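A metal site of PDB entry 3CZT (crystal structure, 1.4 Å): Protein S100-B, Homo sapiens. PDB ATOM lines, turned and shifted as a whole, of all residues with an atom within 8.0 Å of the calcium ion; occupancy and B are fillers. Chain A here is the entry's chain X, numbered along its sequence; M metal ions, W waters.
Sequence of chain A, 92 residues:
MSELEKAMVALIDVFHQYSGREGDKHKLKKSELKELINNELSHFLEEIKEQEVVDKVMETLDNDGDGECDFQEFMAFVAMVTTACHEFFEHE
OD1 of Asp 62 binds the calcium ion, at 2.3 Å.
OD2 of Asp 64 binds the calcium ion (2.3 Å).
O of Glu 68 binds the calcium ion (2.4 Å).
OD1 of Asp 66 is bound to the calcium ion, at 2.4 Å.
OE1 of Glu 73 binds the calcium ion (2.5 Å).
The calcium ion is bound by water W1, 2.5 Å away.
OE2 of Glu 73 binds the calcium ion (2.6 Å).
Five residues have an atom within 4 Å of the calcium ion: Asp 62, Asp 64, Asp 66, Glu 68 and Glu 73.
Along chain A the residues within 4 Å of the calcium ion span positions 62 to 73.
The nearest printed residue that does not touch the calcium ion is Cys 69 (4.4 Å).
The side-chain amino group (NZ) of Lys 27 is in salt-bridge range of the side-chain carboxylate (OD2) of Asp 66 (2.7 Å).
N of Glu 73 sits at hydrogen-bond distance from OD1 of Asp 70, 2.8 Å away.
N of Gly 67 is in hydrogen-bond range of OD2 of Asp 62 (2.7 Å).
The side-chain carboxylate of Glu 73 lies close to the backbone NH of Asn 63.
The side-chain carboxylate of Asp 62 lies close to the backbone NH of Gly 65, at 3.2 Å.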
ATOM      1  N   LYS A  27     -23.102  20.487 -19.861  1.00  0.00           N
ATOM      2  CA  LYS A  27     -23.638  20.581 -21.211  1.00  0.00           C
ATOM      3  C   LYS A  27     -22.744  21.403 -22.111  1.00  0.00           C
ATOM      4  O   LYS A  27     -22.079  22.278 -21.662  1.00  0.00           O
ATOM      5  CB  LYS A  27     -25.043  21.163 -21.226  1.00  0.00           C
ATOM      6  CG  LYS A  27     -26.118  20.453 -20.402  1.00  0.00           C
ATOM      7  CD  LYS A  27     -27.490  21.146 -20.518  1.00  0.00           C
ATOM      8  CE  LYS A  27     -28.567  20.508 -19.596  1.00  0.00           C
ATOM      9  NZ  LYS A  27     -29.871  21.297 -19.682  1.00  0.00           N
ATOM     10  N   LEU A  28     -22.756  21.055 -23.398  1.00  0.00           N
ATOM     11  CA  LEU A  28     -22.074  21.819 -24.467  1.00  0.00           C
ATOM     12  C   LEU A  28     -22.995  22.833 -25.106  1.00  0.00           C
ATOM     13  O   LEU A  28     -24.005  22.466 -25.670  1.00  0.00           O
ATOM     14  CB  LEU A  28     -21.559  20.879 -25.568  1.00  0.00           C
ATOM     15  CG  LEU A  28     -20.581  19.791 -25.143  1.00  0.00           C
ATOM     16  CD1 LEU A  28     -20.522  18.714 -26.232  1.00  0.00           C
ATOM     17  CD2 LEU A  28     -19.209  20.376 -24.959  1.00  0.00           C
ATOM     18  N   MET A  58     -25.951  21.477 -33.934  1.00  0.00           N
ATOM     19  CA  MET A  58     -26.578  21.493 -32.627  1.00  0.00           C
ATOM     20  C   MET A  58     -28.065  21.085 -32.759  1.00  0.00           C
ATOM     21  O   MET A  58     -28.592  20.321 -31.969  1.00  0.00           O
ATOM     22  CB  MET A  58     -26.503  22.882 -31.945  1.00  0.00           C
ATOM     23  CG  MET A  58     -27.265  22.918 -30.607  1.00  0.00           C
ATOM     24  SD  MET A  58     -26.452  21.932 -29.339  1.00  0.00           S
ATOM     25  CE  MET A  58     -25.105  22.965 -28.859  1.00  0.00           C
ATOM     26  N   LEU A  61     -28.342  17.311 -33.155  1.00  0.00           N
ATOM     27  CA  LEU A  61     -28.025  16.449 -31.953  1.00  0.00           C
ATOM     28  C   LEU A  61     -28.825  16.715 -30.698  1.00  0.00           C
ATOM     29  O   LEU A  61     -28.824  15.930 -29.777  1.00  0.00           O
ATOM     30  CB  LEU A  61     -26.549  16.450 -31.668  1.00  0.00           C
ATOM     31  CG  LEU A  61     -25.900  17.711 -31.228  1.00  0.00           C
ATOM     32  CD1 LEU A  61     -26.406  18.171 -29.821  1.00  0.00           C
ATOM     33  CD2 LEU A  61     -24.371  17.409 -31.223  1.00  0.00           C
ATOM     34  N   ASP A  62     -29.546  17.834 -30.676  1.00  0.00           N
ATOM     35  CA  ASP A  62     -30.234  18.334 -29.506  1.00  0.00           C
ATOM     36  C   ASP A  62     -31.635  17.763 -29.368  1.00  0.00           C
ATOM     37  O   ASP A  62     -32.654  18.464 -29.647  1.00  0.00           O
ATOM     38  CB  ASP A  62     -30.332  19.874 -29.524  1.00  0.00           C
ATOM     39  CG  ASP A  62     -31.055  20.426 -28.307  1.00  0.00           C
ATOM     40  OD1 ASP A  62     -31.140  19.749 -27.264  1.00  0.00           O
ATOM     41  OD2 ASP A  62     -31.571  21.557 -28.395  1.00  0.00           O
ATOM     42  N   ASN A  63     -31.717  16.562 -28.856  1.00  0.00           N
ATOM     43  CA  ASN A  63     -33.003  15.880 -28.845  1.00  0.00           C
ATOM     44  C   ASN A  63     -33.999  16.435 -27.858  1.00  0.00           C
ATOM     45  O   ASN A  63     -35.166  16.276 -28.124  1.00  0.00           O
ATOM     46  CB  ASN A  63     -32.811  14.403 -28.602  1.00  0.00           C
ATOM     47  CG  ASN A  63     -31.984  13.772 -29.687  1.00  0.00           C
ATOM     48  OD1 ASN A  63     -31.995  14.200 -30.866  1.00  0.00           O
ATOM     49  ND2 ASN A  63     -31.203  12.775 -29.295  1.00  0.00           N
ATOM     50  N   ASP A  64     -33.590  17.032 -26.747  1.00  0.00           N
ATOM     51  CA  ASP A  64     -34.536  17.616 -25.760  1.00  0.00           C
ATOM     52  C   ASP A  64     -34.831  19.107 -25.904  1.00  0.00           C
ATOM     53  O   ASP A  64     -35.500  19.730 -25.035  1.00  0.00           O
ATOM     54  CB  ASP A  64     -34.164  17.290 -24.321  1.00  0.00           C
ATOM     55  CG  ASP A  64     -32.974  18.060 -23.806  1.00  0.00           C
ATOM     56  OD1 ASP A  64     -32.694  17.969 -22.581  1.00  0.00           O
ATOM     57  OD2 ASP A  64     -32.305  18.757 -24.605  1.00  0.00           O
ATOM     58  N   GLY A  65     -34.312  19.716 -26.961  1.00  0.00           N
ATOM     59  CA  GLY A  65     -34.659  21.100 -27.338  1.00  0.00           C
ATOM     60  C   GLY A  65     -34.133  22.231 -26.496  1.00  0.00           C
ATOM     61  O   GLY A  65     -34.563  23.393 -26.621  1.00  0.00           O
ATOM     62  N   ASP A  66     -33.210  21.934 -25.591  1.00  0.00           N
ATOM     63  CA  ASP A  66     -32.703  22.958 -24.678  1.00  0.00           C
ATOM     64  C   ASP A  66     -31.603  23.823 -25.284  1.00  0.00           C
ATOM     65  O   ASP A  66     -31.077  24.761 -24.690  1.00  0.00           O
ATOM     66  CB  ASP A  66     -32.314  22.385 -23.300  1.00  0.00           C
ATOM     67  CG  ASP A  66     -31.034  21.592 -23.340  1.00  0.00           C
ATOM     68  OD1 ASP A  66     -30.616  21.256 -24.443  1.00  0.00           O
ATOM     69  OD2 ASP A  66     -30.464  21.348 -22.274  1.00  0.00           O
ATOM     70  N   GLY A  67     -31.258  23.532 -26.528  1.00  0.00           N
ATOM     71  CA  GLY A  67     -30.221  24.313 -27.207  1.00  0.00           C
ATOM     72  C   GLY A  67     -28.779  23.986 -26.828  1.00  0.00           C
ATOM     73  O   GLY A  67     -27.853  24.666 -27.263  1.00  0.00           O
ATOM     74  N   GLU A  68     -28.599  22.910 -26.062  1.00  0.00           N
ATOM     75  CA  GLU A  68     -27.271  22.427 -25.666  1.00  0.00           C
ATOM     76  C   GLU A  68     -27.204  20.943 -25.879  1.00  0.00           C
ATOM     77  O   GLU A  68     -28.226  20.259 -26.041  1.00  0.00           O
ATOM     78  CB  GLU A  68     -26.999  22.772 -24.201  1.00  0.00           C
ATOM     79  CG  GLU A  68     -27.119  24.256 -23.891  1.00  0.00           C
ATOM     80  CD  GLU A  68     -26.350  24.688 -22.682  1.00  0.00           C
ATOM     81  OE1 GLU A  68     -25.194  24.214 -22.524  1.00  0.00           O
ATOM     82  OE2 GLU A  68     -26.907  25.495 -21.897  1.00  0.00           O
ATOM     83  N   CYS A  69     -25.978  20.437 -25.871  1.00  0.00           N
ATOM     84  CA  CYS A  69     -25.725  19.015 -25.951  1.00  0.00           C
ATOM     85  C   CYS A  69     -25.334  18.499 -24.595  1.00  0.00           C
ATOM     86  O   CYS A  69     -24.295  18.830 -24.102  1.00  0.00           O
ATOM     87  CB  CYS A  69     -24.620  18.713 -26.986  1.00  0.00           C
ATOM     88  SG  CYS A  69     -24.265  17.047 -27.251  1.00  0.00           S
ATOM     89  N   ASP A  70     -26.156  17.617 -24.033  1.00  0.00           N
ATOM     90  CA  ASP A  70     -25.855  16.983 -22.767  1.00  0.00           C
ATOM     91  C   ASP A  70     -25.048  15.687 -22.999  1.00  0.00           C
ATOM     92  O   ASP A  70     -24.705  15.355 -24.144  1.00  0.00           O
ATOM     93  CB  ASP A  70     -27.132  16.786 -21.908  1.00  0.00           C
ATOM     94  CG  ASP A  70     -28.091  15.731 -22.439  1.00  0.00           C
ATOM     95  OD1 ASP A  70     -27.767  14.973 -23.375  1.00  0.00           O
ATOM     96  OD2 ASP A  70     -29.210  15.665 -21.875  1.00  0.00           O
ATOM     97  N   PHE A  71     -24.794  14.955 -21.924  1.00  0.00           N
ATOM     98  CA  PHE A  71     -23.950  13.782 -22.044  1.00  0.00           C
ATOM     99  C   PHE A  71     -24.560  12.714 -22.940  1.00  0.00           C
ATOM    100  O   PHE A  71     -23.895  12.154 -23.853  1.00  0.00           O
ATOM    101  CB  PHE A  71     -23.613  13.223 -20.654  1.00  0.00           C
ATOM    102  CG  PHE A  71     -22.578  12.143 -20.686  1.00  0.00           C
ATOM    103  CD1 PHE A  71     -21.256  12.452 -20.771  1.00  0.00           C
ATOM    104  CD2 PHE A  71     -22.938  10.816 -20.697  1.00  0.00           C
ATOM    105  CE1 PHE A  71     -20.307  11.493 -20.828  1.00  0.00           C
ATOM    106  CE2 PHE A  71     -22.008   9.843 -20.774  1.00  0.00           C
ATOM    107  CZ  PHE A  71     -20.692  10.164 -20.800  1.00  0.00           C
ATOM    108  N   GLU A  73     -26.777  13.116 -25.260  1.00  0.00           N
ATOM    109  CA  GLU A  73     -26.750  13.600 -26.660  1.00  0.00           C
ATOM    110  C   GLU A  73     -25.325  13.559 -27.257  1.00  0.00           C
ATOM    111  O   GLU A  73     -25.140  13.309 -28.427  1.00  0.00           O
ATOM    112  CB  GLU A  73     -27.320  14.997 -26.707  1.00  0.00           C
ATOM    113  CG  GLU A  73     -28.827  15.056 -26.495  1.00  0.00           C
ATOM    114  CD  GLU A  73     -29.337  16.415 -26.053  1.00  0.00           C
ATOM    115  OE1 GLU A  73     -28.514  17.289 -25.739  1.00  0.00           O
ATOM    116  OE2 GLU A  73     -30.581  16.666 -26.012  1.00  0.00           O
ATOM    117  N   PHE A  74     -24.317  13.793 -26.440  1.00  0.00           N
ATOM    118  CA  PHE A  74     -22.933  13.702 -26.877  1.00  0.00           C
ATOM    119  C   PHE A  74     -22.587  12.247 -27.216  1.00  0.00           C
ATOM    120  O   PHE A  74     -21.945  11.988 -28.256  1.00  0.00           O
ATOM    121  CB  PHE A  74     -21.995  14.214 -25.806  1.00  0.00           C
ATOM    122  CG  PHE A  74     -20.565  14.109 -26.204  1.00  0.00           C
ATOM    123  CD1 PHE A  74     -20.080  14.911 -27.222  1.00  0.00           C
ATOM    124  CD2 PHE A  74     -19.683  13.240 -25.568  1.00  0.00           C
ATOM    125  CE1 PHE A  74     -18.759  14.827 -27.638  1.00  0.00           C
ATOM    126  CE2 PHE A  74     -18.360  13.173 -25.997  1.00  0.00           C
ATOM    127  CZ  PHE A  74     -17.904  13.985 -27.021  1.00  0.00           C
HETATM  128 CA    CA M   1     -30.139  19.079 -25.308  1.00  0.00          CA
HETATM  129  O   HOH W   1     -29.479  18.919 -22.942  1.00  0.00           O
